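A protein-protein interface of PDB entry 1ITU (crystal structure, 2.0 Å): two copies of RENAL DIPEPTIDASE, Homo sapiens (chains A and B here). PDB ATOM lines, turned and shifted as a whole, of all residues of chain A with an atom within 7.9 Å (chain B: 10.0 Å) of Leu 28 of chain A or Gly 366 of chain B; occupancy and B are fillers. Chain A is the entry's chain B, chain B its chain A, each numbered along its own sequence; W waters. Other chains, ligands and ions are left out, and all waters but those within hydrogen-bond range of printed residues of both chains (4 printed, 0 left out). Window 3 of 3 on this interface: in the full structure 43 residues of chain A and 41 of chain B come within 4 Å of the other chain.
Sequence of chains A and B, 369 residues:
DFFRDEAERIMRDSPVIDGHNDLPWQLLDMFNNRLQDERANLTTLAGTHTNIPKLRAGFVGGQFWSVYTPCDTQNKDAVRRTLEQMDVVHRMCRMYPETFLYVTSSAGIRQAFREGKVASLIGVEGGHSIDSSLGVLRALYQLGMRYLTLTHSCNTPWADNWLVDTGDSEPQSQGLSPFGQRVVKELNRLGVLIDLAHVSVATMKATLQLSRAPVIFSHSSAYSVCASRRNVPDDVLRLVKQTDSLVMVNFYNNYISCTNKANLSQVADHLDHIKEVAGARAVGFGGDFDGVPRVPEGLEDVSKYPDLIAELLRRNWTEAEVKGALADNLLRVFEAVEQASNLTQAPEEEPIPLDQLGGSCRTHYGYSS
Water W3 lies within hydrogen-bond range of O of Glu 349 of chain B and O of Asn 32 of chain A.
Leu 28 of chain A touches just these residues of chain B: Tyr 365 (3.97 Å) and Gly 366 (3.2 Å).
Of chain A, only Leu 28 and Asn 32 come within 4 Å of Gly 366 of chain B.
No residue of chain B comes within 4 Å of Asp 29 of chain A.
Of the printed residues of chain A, Glu 349 of chain B touches Asn 33, Arg 34 and Leu 35.
Of the printed residues of chain B, Arg 34 of chain A touches Glu 349 (3.2 Å).
The nearest residue of chain B that does not touch Leu 28 of chain A is Tyr 367 of chain B (5.3 Å).
The nearest printed residue of chain A that does not touch Thr 363 of chain B is Arg 80 of chain A (5.7 Å).
Hydrophobic or aromatic side chains of chain B that line the printed part of chain A: Pro 351, Tyr 365 and Tyr 367.
Of the 22 printed residues of chain A, 10 touch a printed residue of chain B.
Hydrophobic or aromatic side chains of chain A that line the printed part of chain B: Trp 25, Leu 28, Leu 35 and Pro 70.
Among the printed residues, no Asp or Glu carboxylate lies within 4 Å of a Lys or Arg side-chain nitrogen of the other chain.
The side-chain carboxylate (OE2) of Glu 349 of chain B lies within hydrogen-bond range of the backbone NH (N) of Leu 35 of chain A (3.0 Å).
The guanidinium group of Arg 81 of chain A sits at hydrogen-bond distance from the backbone carbonyl oxygen of Tyr 365 of chain B (3.1 Å).
OE2 of Glu 84 of chain A is in hydrogen-bond range of OG of Ser 133 of chain B, 2.6 Å away.
The backbone carbonyl oxygen (O) of Thr 363 of chain B sits at hydrogen-bond distance from the guanidinium group (NH1) of Arg 81 of chain A, at 2.6 Å.
The backbone carbonyl oxygen (O) of Gly 366 of chain B lies close to the side-chain amide nitrogen (ND2) of Asn 32 of chain A, at 3.4 Å.
No position is printed for both chains.
Of the 15 pairs that touch across the chains among the printed residues, none has its exchanged pair printed and touching as well.
The backbone NH of Leu 28 of chain A sits at hydrogen-bond distance from the side-chain amide oxygen of Asn 33 of chain A (3.1 Å).
O of Leu 27 of chain A is in hydrogen-bond range of N of Asn 33 of chain A, at 3.1 Å.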
ATOM      1  N   ASP A  22      18.788  13.428  37.230  1.00  0.00           N
ATOM      2  CA  ASP A  22      18.967  13.945  35.877  1.00  0.00           C
ATOM      3  C   ASP A  22      20.355  13.746  35.303  1.00  0.00           C
ATOM      4  O   ASP A  22      20.859  14.629  34.610  1.00  0.00           O
ATOM      5  CB  ASP A  22      18.627  15.427  35.796  1.00  0.00           C
ATOM      6  CG  ASP A  22      17.162  15.674  35.611  1.00  0.00           C
ATOM      7  OD1 ASP A  22      16.572  16.333  36.496  1.00  0.00           O
ATOM      8  OD2 ASP A  22      16.599  15.242  34.579  1.00  0.00           O
ATOM      9  N   LEU A  23      20.982  12.608  35.589  1.00  0.00           N
ATOM     10  CA  LEU A  23      22.309  12.339  35.036  1.00  0.00           C
ATOM     11  C   LEU A  23      22.261  12.368  33.495  1.00  0.00           C
ATOM     12  O   LEU A  23      23.093  13.016  32.869  1.00  0.00           O
ATOM     13  CB  LEU A  23      22.866  10.997  35.544  1.00  0.00           C
ATOM     14  CG  LEU A  23      24.242  10.526  35.025  1.00  0.00           C
ATOM     15  CD1 LEU A  23      25.308  11.579  35.273  1.00  0.00           C
ATOM     16  CD2 LEU A  23      24.635   9.225  35.689  1.00  0.00           C
ATOM     17  N   PRO A  24      21.243  11.725  32.870  1.00  0.00           N
ATOM     18  CA  PRO A  24      21.160  11.729  31.402  1.00  0.00           C
ATOM     19  C   PRO A  24      21.291  13.127  30.806  1.00  0.00           C
ATOM     20  O   PRO A  24      22.001  13.326  29.810  1.00  0.00           O
ATOM     21  CB  PRO A  24      19.783  11.117  31.145  1.00  0.00           C
ATOM     22  CG  PRO A  24      19.659  10.136  32.245  1.00  0.00           C
ATOM     23  CD  PRO A  24      20.166  10.890  33.443  1.00  0.00           C
ATOM     24  N   TRP A  25      20.641  14.092  31.456  1.00  0.00           N
ATOM     25  CA  TRP A  25      20.666  15.492  31.043  1.00  0.00           C
ATOM     26  C   TRP A  25      22.089  16.049  31.040  1.00  0.00           C
ATOM     27  O   TRP A  25      22.454  16.817  30.154  1.00  0.00           O
ATOM     28  CB  TRP A  25      19.784  16.337  31.973  1.00  0.00           C
ATOM     29  CG  TRP A  25      19.885  17.793  31.697  1.00  0.00           C
ATOM     30  CD1 TRP A  25      20.422  18.744  32.509  1.00  0.00           C
ATOM     31  CD2 TRP A  25      19.511  18.459  30.487  1.00  0.00           C
ATOM     32  NE1 TRP A  25      20.419  19.963  31.876  1.00  0.00           N
ATOM     33  CE2 TRP A  25      19.864  19.815  30.632  1.00  0.00           C
ATOM     34  CE3 TRP A  25      18.914  18.038  29.287  1.00  0.00           C
ATOM     35  CZ2 TRP A  25      19.644  20.757  29.622  1.00  0.00           C
ATOM     36  CZ3 TRP A  25      18.695  18.971  28.289  1.00  0.00           C
ATOM     37  CH2 TRP A  25      19.061  20.316  28.461  1.00  0.00           C
ATOM     38  N   GLN A  26      22.880  15.680  32.047  1.00  0.00           N
ATOM     39  CA  GLN A  26      24.270  16.128  32.147  1.00  0.00           C
ATOM     40  C   GLN A  26      25.113  15.508  31.031  1.00  0.00           C
ATOM     41  O   GLN A  26      25.980  16.172  30.458  1.00  0.00           O
ATOM     42  CB  GLN A  26      24.864  15.753  33.510  1.00  0.00           C
ATOM     43  CG  GLN A  26      24.168  16.405  34.685  1.00  0.00           C
ATOM     44  CD  GLN A  26      24.148  17.917  34.569  1.00  0.00           C
ATOM     45  OE1 GLN A  26      25.120  18.525  34.121  1.00  0.00           O
ATOM     46  NE2 GLN A  26      23.031  18.532  34.953  1.00  0.00           N
ATOM     47  N   LEU A  27      24.853  14.231  30.739  1.00  0.00           N
ATOM     48  CA  LEU A  27      25.576  13.510  29.691  1.00  0.00           C
ATOM     49  C   LEU A  27      25.348  14.196  28.351  1.00  0.00           C
ATOM     50  O   LEU A  27      26.262  14.304  27.545  1.00  0.00           O
ATOM     51  CB  LEU A  27      25.144  12.044  29.639  1.00  0.00           C
ATOM     52  CG  LEU A  27      25.432  11.243  30.915  1.00  0.00           C
ATOM     53  CD1 LEU A  27      24.914   9.819  30.784  1.00  0.00           C
ATOM     54  CD2 LEU A  27      26.927  11.260  31.219  1.00  0.00           C
ATOM     55  N   LEU A  28      24.130  14.688  28.138  1.00  0.00           N
ATOM     56  CA  LEU A  28      23.787  15.404  26.919  1.00  0.00           C
ATOM     57  C   LEU A  28      24.479  16.767  26.906  1.00  0.00           C
ATOM     58  O   LEU A  28      25.136  17.143  25.935  1.00  0.00           O
ATOM     59  CB  LEU A  28      22.270  15.624  26.836  1.00  0.00           C
ATOM     60  CG  LEU A  28      21.811  16.677  25.814  1.00  0.00           C
ATOM     61  CD1 LEU A  28      22.151  16.220  24.398  1.00  0.00           C
ATOM     62  CD2 LEU A  28      20.317  16.940  25.934  1.00  0.00           C
ATOM     63  N   ASP A  29      24.309  17.502  27.997  1.00  0.00           N
ATOM     64  CA  ASP A  29      24.870  18.836  28.133  1.00  0.00           C
ATOM     65  C   ASP A  29      26.387  18.874  28.144  1.00  0.00           C
ATOM     66  O   ASP A  29      26.989  19.748  27.523  1.00  0.00           O
ATOM     67  CB  ASP A  29      24.323  19.504  29.398  1.00  0.00           C
ATOM     68  CG  ASP A  29      24.687  20.970  29.485  1.00  0.00           C
ATOM     69  OD1 ASP A  29      25.432  21.345  30.418  1.00  0.00           O
ATOM     70  OD2 ASP A  29      24.227  21.745  28.619  1.00  0.00           O
ATOM     71  N   MET A  30      27.001  17.920  28.832  1.00  0.00           N
ATOM     72  CA  MET A  30      28.453  17.876  28.937  1.00  0.00           C
ATOM     73  C   MET A  30      29.197  17.179  27.798  1.00  0.00           C
ATOM     74  O   MET A  30      30.306  17.593  27.456  1.00  0.00           O
ATOM     75  CB  MET A  30      28.871  17.217  30.254  1.00  0.00           C
ATOM     76  CG  MET A  30      28.463  17.960  31.510  1.00  0.00           C
ATOM     77  SD  MET A  30      28.849  16.977  32.969  1.00  0.00           S
ATOM     78  CE  MET A  30      30.621  17.092  33.004  1.00  0.00           C
ATOM     79  N   PHE A  31      28.613  16.126  27.223  1.00  0.00           N
ATOM     80  CA  PHE A  31      29.300  15.364  26.168  1.00  0.00           C
ATOM     81  C   PHE A  31      28.506  15.069  24.896  1.00  0.00           C
ATOM     82  O   PHE A  31      28.975  14.309  24.056  1.00  0.00           O
ATOM     83  CB  PHE A  31      29.797  14.018  26.731  1.00  0.00           C
ATOM     84  CG  PHE A  31      30.324  14.094  28.136  1.00  0.00           C
ATOM     85  CD1 PHE A  31      31.570  14.656  28.401  1.00  0.00           C
ATOM     86  CD2 PHE A  31      29.568  13.610  29.201  1.00  0.00           C
ATOM     87  CE1 PHE A  31      32.053  14.737  29.710  1.00  0.00           C
ATOM     88  CE2 PHE A  31      30.042  13.684  30.509  1.00  0.00           C
ATOM     89  CZ  PHE A  31      31.286  14.248  30.764  1.00  0.00           C
ATOM     90  N   ASN A  32      27.313  15.646  24.767  1.00  0.00           N
ATOM     91  CA  ASN A  32      26.437  15.425  23.613  1.00  0.00           C
ATOM     92  C   ASN A  32      26.130  13.930  23.504  1.00  0.00           C
ATOM     93  O   ASN A  32      26.100  13.356  22.412  1.00  0.00           O
ATOM     94  CB  ASN A  32      27.077  15.962  22.318  1.00  0.00           C
ATOM     95  CG  ASN A  32      26.038  16.409  21.290  1.00  0.00           C
ATOM     96  OD1 ASN A  32      24.834  16.282  21.511  1.00  0.00           O
ATOM     97  ND2 ASN A  32      26.503  16.960  20.178  1.00  0.00           N
ATOM     98  N   ASN A  33      25.961  13.304  24.669  1.00  0.00           N
ATOM     99  CA  ASN A  33      25.667  11.878  24.800  1.00  0.00           C
ATOM    100  C   ASN A  33      26.718  10.915  24.243  1.00  0.00           C
ATOM    101  O   ASN A  33      26.409   9.769  23.905  1.00  0.00           O
ATOM    102  CB  ASN A  33      24.276  11.565  24.248  1.00  0.00           C
ATOM    103  CG  ASN A  33      23.175  12.136  25.118  1.00  0.00           C
ATOM    104  OD1 ASN A  33      23.351  12.306  26.328  1.00  0.00           O
ATOM    105  ND2 ASN A  33      22.034  12.433  24.511  1.00  0.00           N
ATOM    106  N   ARG A  34      27.965  11.381  24.170  1.00  0.00           N
ATOM    107  CA  ARG A  34      29.066  10.554  23.693  1.00  0.00           C
ATOM    108  C   ARG A  34      29.666   9.842  24.904  1.00  0.00           C
ATOM    109  O   ARG A  34      30.600  10.339  25.539  1.00  0.00           O
ATOM    110  CB  ARG A  34      30.107  11.412  22.973  1.00  0.00           C
ATOM    111  CG  ARG A  34      29.494  12.219  21.843  1.00  0.00           C
ATOM    112  CD  ARG A  34      30.523  12.998  21.079  1.00  0.00           C
ATOM    113  NE  ARG A  34      31.388  12.104  20.319  1.00  0.00           N
ATOM    114  CZ  ARG A  34      32.008  12.432  19.186  1.00  0.00           C
ATOM    115  NH1 ARG A  34      32.774  11.539  18.569  1.00  0.00           N
ATOM    116  NH2 ARG A  34      31.868  13.648  18.668  1.00  0.00           N
ATOM    117  N   LEU A  35      29.108   8.672  25.212  1.00  0.00           N
ATOM    118  CA  LEU A  35      29.524   7.870  26.357  1.00  0.00           C
ATOM    119  C   LEU A  35      30.930   7.291  26.264  1.00  0.00           C
ATOM    120  O   LEU A  35      31.505   6.861  27.274  1.00  0.00           O
ATOM    121  CB  LEU A  35      28.502   6.758  26.613  1.00  0.00           C
ATOM    122  CG  LEU A  35      27.072   7.235  26.890  1.00  0.00           C
ATOM    123  CD1 LEU A  35      26.191   6.051  27.184  1.00  0.00           C
ATOM    124  CD2 LEU A  35      27.056   8.217  28.051  1.00  0.00           C
ATOM    125  N   TYR A  68      14.668  13.821  30.317  1.00  0.00           N
ATOM    126  CA  TYR A  68      14.167  15.174  30.273  1.00  0.00           C
ATOM    127  C   TYR A  68      14.635  16.005  29.091  1.00  0.00           C
ATOM    128  O   TYR A  68      15.820  16.058  28.784  1.00  0.00           O
ATOM    129  CB  TYR A  68      14.552  15.879  31.589  1.00  0.00           C
ATOM    130  CG  TYR A  68      14.515  17.395  31.547  1.00  0.00           C
ATOM    131  CD1 TYR A  68      15.685  18.136  31.362  1.00  0.00           C
ATOM    132  CD2 TYR A  68      13.306  18.090  31.688  1.00  0.00           C
ATOM    133  CE1 TYR A  68      15.651  19.532  31.318  1.00  0.00           C
ATOM    134  CE2 TYR A  68      13.264  19.478  31.644  1.00  0.00           C
ATOM    135  CZ  TYR A  68      14.433  20.192  31.461  1.00  0.00           C
ATOM    136  OH  TYR A  68      14.384  21.558  31.408  1.00  0.00           O
ATOM    137  N   THR A  69      13.675  16.674  28.463  1.00  0.00           N
ATOM    138  CA  THR A  69      13.925  17.575  27.351  1.00  0.00           C
ATOM    139  C   THR A  69      13.270  18.884  27.815  1.00  0.00           C
ATOM    140  O   THR A  69      12.154  18.873  28.341  1.00  0.00           O
ATOM    141  CB  THR A  69      13.319  17.029  26.025  1.00  0.00           C
ATOM    142  OG1 THR A  69      13.623  17.938  24.967  1.00  0.00           O
ATOM    143  CG2 THR A  69      11.814  16.848  26.120  1.00  0.00           C
ATOM    144  N   PRO A  70      13.988  20.015  27.711  1.00  0.00           N
ATOM    145  CA  PRO A  70      13.475  21.326  28.135  1.00  0.00           C
ATOM    146  C   PRO A  70      12.149  21.759  27.533  1.00  0.00           C
ATOM    147  O   PRO A  70      11.781  21.337  26.438  1.00  0.00           O
ATOM    148  CB  PRO A  70      14.598  22.278  27.738  1.00  0.00           C
ATOM    149  CG  PRO A  70      15.818  21.412  27.860  1.00  0.00           C
ATOM    150  CD  PRO A  70      15.359  20.145  27.193  1.00  0.00           C
ATOM    151  N   ARG A  80      12.077  13.985  19.368  1.00  0.00           N
ATOM    152  CA  ARG A  80      13.419  13.554  18.952  1.00  0.00           C
ATOM    153  C   ARG A  80      14.358  13.456  20.161  1.00  0.00           C
ATOM    154  O   ARG A  80      14.984  12.428  20.394  1.00  0.00           O
ATOM    155  CB  ARG A  80      14.005  14.563  17.963  1.00  0.00           C
ATOM    156  CG  ARG A  80      15.401  14.220  17.435  1.00  0.00           C
ATOM    157  CD  ARG A  80      15.988  15.456  16.773  1.00  0.00           C
ATOM    158  NE  ARG A  80      17.170  15.187  15.959  1.00  0.00           N
ATOM    159  CZ  ARG A  80      18.417  15.458  16.337  1.00  0.00           C
ATOM    160  NH1 ARG A  80      19.438  15.185  15.521  1.00  0.00           N
ATOM    161  NH2 ARG A  80      18.650  15.981  17.543  1.00  0.00           N
ATOM    162  N   ARG A  81      14.436  14.527  20.939  1.00  0.00           N
ATOM    163  CA  ARG A  81      15.309  14.546  22.108  1.00  0.00           C
ATOM    164  C   ARG A  81      14.921  13.581  23.223  1.00  0.00           C
ATOM    165  O   ARG A  81      15.789  13.101  23.945  1.00  0.00           O
ATOM    166  CB  ARG A  81      15.481  15.968  22.638  1.00  0.00           C
ATOM    167  CG  ARG A  81      16.163  16.870  21.630  1.00  0.00           C
ATOM    168  CD  ARG A  81      16.691  18.146  22.283  1.00  0.00           C
ATOM    169  NE  ARG A  81      17.540  18.901  21.364  1.00  0.00           N
ATOM    170  CZ  ARG A  81      18.801  18.584  21.081  1.00  0.00           C
ATOM    171  NH1 ARG A  81      19.496  19.322  20.228  1.00  0.00           N
ATOM    172  NH2 ARG A  81      19.375  17.535  21.661  1.00  0.00           N
ATOM    173  N   GLU A  84      16.401  10.326  22.137  1.00  0.00           N
ATOM    174  CA  GLU A  84      17.842  10.349  22.349  1.00  0.00           C
ATOM    175  C   GLU A  84      18.189  10.199  23.825  1.00  0.00           C
ATOM    176  O   GLU A  84      19.191   9.576  24.164  1.00  0.00           O
ATOM    177  CB  GLU A  84      18.438  11.647  21.839  1.00  0.00           C
ATOM    178  CG  GLU A  84      18.241  11.867  20.367  1.00  0.00           C
ATOM    179  CD  GLU A  84      18.980  13.085  19.889  1.00  0.00           C
ATOM    180  OE1 GLU A  84      18.920  14.134  20.567  1.00  0.00           O
ATOM    181  OE2 GLU A  84      19.645  12.993  18.843  1.00  0.00           O
ATOM    182  N   GLN A  85      17.379  10.792  24.705  1.00  0.00           N
ATOM    183  CA  GLN A  85      17.643  10.678  26.138  1.00  0.00           C
ATOM    184  C   GLN A  85      17.364   9.272  26.656  1.00  0.00           C
ATOM    185  O   GLN A  85      18.116   8.749  27.482  1.00  0.00           O
ATOM    186  CB  GLN A  85      16.886  11.752  26.931  1.00  0.00           C
ATOM    187  CG  GLN A  85      17.366  13.169  26.618  1.00  0.00           C
ATOM    188  CD  GLN A  85      18.894  13.286  26.623  1.00  0.00           C
ATOM    189  OE1 GLN A  85      19.539  13.336  25.561  1.00  0.00           O
ATOM    190  NE2 GLN A  85      19.479  13.317  27.815  1.00  0.00           N
ATOM    191  N   VAL A  88      20.294   7.221  25.561  1.00  0.00           N
ATOM    192  CA  VAL A  88      21.490   7.321  26.391  1.00  0.00           C
ATOM    193  C   VAL A  88      21.371   6.466  27.656  1.00  0.00           C
ATOM    194  O   VAL A  88      22.363   5.907  28.119  1.00  0.00           O
ATOM    195  CB  VAL A  88      21.913   8.794  26.699  1.00  0.00           C
ATOM    196  CG1 VAL A  88      21.169   9.362  27.899  1.00  0.00           C
ATOM    197  CG2 VAL A  88      23.411   8.844  26.961  1.00  0.00           C
ATOM    198  N   SER B 133      19.361  11.714  13.712  1.00  0.00           N
ATOM    199  CA  SER B 133      19.774  11.306  15.048  1.00  0.00           C
ATOM    200  C   SER B 133      19.988   9.814  15.124  1.00  0.00           C
ATOM    201  O   SER B 133      19.107   9.045  14.764  1.00  0.00           O
ATOM    202  CB  SER B 133      18.699  11.704  16.067  1.00  0.00           C
ATOM    203  OG  SER B 133      18.879  11.004  17.287  1.00  0.00           O
ATOM    204  N   GLU B 349      27.991   7.033  17.911  1.00  0.00           N
ATOM    205  CA  GLU B 349      27.526   8.165  18.695  1.00  0.00           C
ATOM    206  C   GLU B 349      28.077   9.515  18.259  1.00  0.00           C
ATOM    207  O   GLU B 349      27.878  10.508  18.948  1.00  0.00           O
ATOM    208  CB  GLU B 349      27.813   7.933  20.180  1.00  0.00           C
ATOM    209  CG  GLU B 349      29.295   7.946  20.525  1.00  0.00           C
ATOM    210  CD  GLU B 349      29.560   7.719  21.994  1.00  0.00           C
ATOM    211  OE1 GLU B 349      30.655   8.093  22.462  1.00  0.00           O
ATOM    212  OE2 GLU B 349      28.684   7.158  22.678  1.00  0.00           O
ATOM    213  N   PRO B 351      27.508  12.492  16.501  1.00  0.00           N
ATOM    214  CA  PRO B 351      26.366  13.169  15.907  1.00  0.00           C
ATOM    215  C   PRO B 351      26.680  13.898  14.610  1.00  0.00           C
ATOM    216  O   PRO B 351      27.841  14.113  14.270  1.00  0.00           O
ATOM    217  CB  PRO B 351      25.966  14.148  17.002  1.00  0.00           C
ATOM    218  CG  PRO B 351      27.300  14.558  17.543  1.00  0.00           C
ATOM    219  CD  PRO B 351      27.996  13.238  17.679  1.00  0.00           C
ATOM    220  N   ILE B 352      25.624  14.254  13.887  1.00  0.00           N
ATOM    221  CA  ILE B 352      25.747  14.997  12.644  1.00  0.00           C
ATOM    222  C   ILE B 352      26.228  16.391  13.043  1.00  0.00           C
ATOM    223  O   ILE B 352      25.894  16.881  14.135  1.00  0.00           O
ATOM    224  CB  ILE B 352      24.365  15.092  11.924  1.00  0.00           C
ATOM    225  CG1 ILE B 352      24.508  15.738  10.547  1.00  0.00           C
ATOM    226  CG2 ILE B 352      23.365  15.907  12.757  1.00  0.00           C
ATOM    227  CD1 ILE B 352      23.199  15.793   9.764  1.00  0.00           C
ATOM    228  N   LEU B 354      26.388  20.125  13.672  1.00  0.00           N
ATOM    229  CA  LEU B 354      25.309  21.091  13.861  1.00  0.00           C
ATOM    230  C   LEU B 354      24.926  21.901  12.617  1.00  0.00           C
ATOM    231  O   LEU B 354      23.747  22.130  12.353  1.00  0.00           O
ATOM    232  CB  LEU B 354      25.680  22.058  14.977  1.00  0.00           C
ATOM    233  CG  LEU B 354      24.706  23.223  15.070  1.00  0.00           C
ATOM    234  CD1 LEU B 354      23.707  22.982  16.169  1.00  0.00           C
ATOM    235  CD2 LEU B 354      25.484  24.497  15.282  1.00  0.00           C
ATOM    236  N   LEU B 357      22.322  20.450  10.119  1.00  0.00           N
ATOM    237  CA  LEU B 357      20.909  20.327  10.482  1.00  0.00           C
ATOM    238  C   LEU B 357      20.125  21.519   9.926  1.00  0.00           C
ATOM    239  O   LEU B 357      20.590  22.659   9.981  1.00  0.00           O
ATOM    240  CB  LEU B 357      20.746  20.256  12.001  1.00  0.00           C
ATOM    241  CG  LEU B 357      21.151  18.953  12.678  1.00  0.00           C
ATOM    242  CD1 LEU B 357      21.098  19.108  14.206  1.00  0.00           C
ATOM    243  CD2 LEU B 357      20.218  17.851  12.227  1.00  0.00           C
ATOM    244  N   THR B 363      16.119  22.539  18.712  1.00  0.00           N
ATOM    245  CA  THR B 363      16.935  23.245  19.686  1.00  0.00           C
ATOM    246  C   THR B 363      18.335  22.628  19.574  1.00  0.00           C
ATOM    247  O   THR B 363      18.482  21.496  19.113  1.00  0.00           O
ATOM    248  CB  THR B 363      16.352  23.115  21.123  1.00  0.00           C
ATOM    249  OG1 THR B 363      16.019  21.747  21.392  1.00  0.00           O
ATOM    250  CG2 THR B 363      15.108  23.984  21.268  1.00  0.00           C
ATOM    251  N   HIS B 364      19.356  23.346  20.021  1.00  0.00           N
ATOM    252  CA  HIS B 364      20.717  22.850  19.879  1.00  0.00           C
ATOM    253  C   HIS B 364      21.459  22.338  21.107  1.00  0.00           C
ATOM    254  O   HIS B 364      22.690  22.424  21.172  1.00  0.00           O
ATOM    255  CB  HIS B 364      21.541  23.881  19.110  1.00  0.00           C
ATOM    256  CG  HIS B 364      20.955  24.226  17.772  1.00  0.00           C
ATOM    257  ND1 HIS B 364      20.878  25.517  17.297  1.00  0.00           N
ATOM    258  CD2 HIS B 364      20.394  23.443  16.818  1.00  0.00           C
ATOM    259  CE1 HIS B 364      20.294  25.516  16.110  1.00  0.00           C
ATOM    260  NE2 HIS B 364      19.991  24.270  15.799  1.00  0.00           N
ATOM    261  N   TYR B 365      20.718  21.729  22.033  1.00  0.00           N
ATOM    262  CA  TYR B 365      21.299  21.158  23.250  1.00  0.00           C
ATOM    263  C   TYR B 365      22.297  20.063  22.893  1.00  0.00           C
ATOM    264  O   TYR B 365      22.102  19.324  21.931  1.00  0.00           O
ATOM    265  CB  TYR B 365      20.211  20.562  24.145  1.00  0.00           C
ATOM    266  CG  TYR B 365      19.243  21.582  24.685  1.00  0.00           C
ATOM    267  CD1 TYR B 365      19.643  22.491  25.662  1.00  0.00           C
ATOM    268  CD2 TYR B 365      17.934  21.659  24.200  1.00  0.00           C
ATOM    269  CE1 TYR B 365      18.768  23.460  26.143  1.00  0.00           C
ATOM    270  CE2 TYR B 365      17.046  22.623  24.671  1.00  0.00           C
ATOM    271  CZ  TYR B 365      17.475  23.525  25.644  1.00  0.00           C
ATOM    272  OH  TYR B 365      16.625  24.500  26.115  1.00  0.00           O
ATOM    273  N   GLY B 366      23.352  19.951  23.691  1.00  0.00           N
ATOM    274  CA  GLY B 366      24.366  18.941  23.449  1.00  0.00           C
ATOM    275  C   GLY B 366      25.518  19.523  22.664  1.00  0.00           C
ATOM    276  O   GLY B 366      26.662  19.111  22.829  1.00  0.00           O
ATOM    277  N   TYR B 367      25.203  20.465  21.785  1.00  0.00           N
ATOM    278  CA  TYR B 367      26.211  21.125  20.966  1.00  0.00           C
ATOM    279  C   TYR B 367      26.542  22.479  21.578  1.00  0.00           C
ATOM    280  O   TYR B 367      27.703  22.760  21.900  1.00  0.00           O
ATOM    281  CB  TYR B 367      25.675  21.407  19.560  1.00  0.00           C
ATOM    282  CG  TYR B 367      25.311  20.216  18.725  1.00  0.00           C
ATOM    283  CD1 TYR B 367      26.282  19.537  17.985  1.00  0.00           C
ATOM    284  CD2 TYR B 367      23.985  19.833  18.586  1.00  0.00           C
ATOM    285  CE1 TYR B 367      25.938  18.517  17.117  1.00  0.00           C
ATOM    286  CE2 TYR B 367      23.625  18.814  17.720  1.00  0.00           C
ATOM    287  CZ  TYR B 367      24.606  18.162  16.983  1.00  0.00           C
ATOM    288  OH  TYR B 367      24.237  17.180  16.095  1.00  0.00           O
ATOM    289  N   SER B 368      25.488  23.301  21.686  1.00  0.00           N
ATOM    290  CA  SER B 368      25.489  24.688  22.185  1.00  0.00           C
ATOM    291  C   SER B 368      25.647  25.643  20.986  1.00  0.00           C
ATOM    292  O   SER B 368      26.773  25.995  20.598  1.00  0.00           O
ATOM    293  CB  SER B 368      26.591  24.943  23.234  1.00  0.00           C
ATOM    294  OG  SER B 368      26.388  24.172  24.411  1.00  0.00           O
ATOM    295  N   SER B 369      24.515  26.027  20.388  1.00  0.00           N
ATOM    296  CA  SER B 369      24.511  26.915  19.221  1.00  0.00           C
ATOM    297  C   SER B 369      23.099  27.232  18.703  1.00  0.00           C
ATOM    298  O   SER B 369      22.188  27.396  19.543  1.00  0.00           O
ATOM    299  CB  SER B 369      25.355  26.297  18.106  1.00  0.00           C
ATOM    300  OG  SER B 369      25.072  24.911  18.004  1.00  0.00           O
ATOM    301  OXT SER B 369      22.915  27.328  17.468  1.00  0.00           O
HETATM  302  O   HOH W   1      32.441   9.402  21.308  1.00  0.00           O
HETATM  303  O   HOH W   2      23.611  21.902  25.889  1.00  0.00           O
HETATM  304  O   HOH W   3      26.001  11.072  20.526  1.00  0.00           O
HETATM  305  O   HOH W   4      21.885  15.963  16.845  1.00  0.00           O
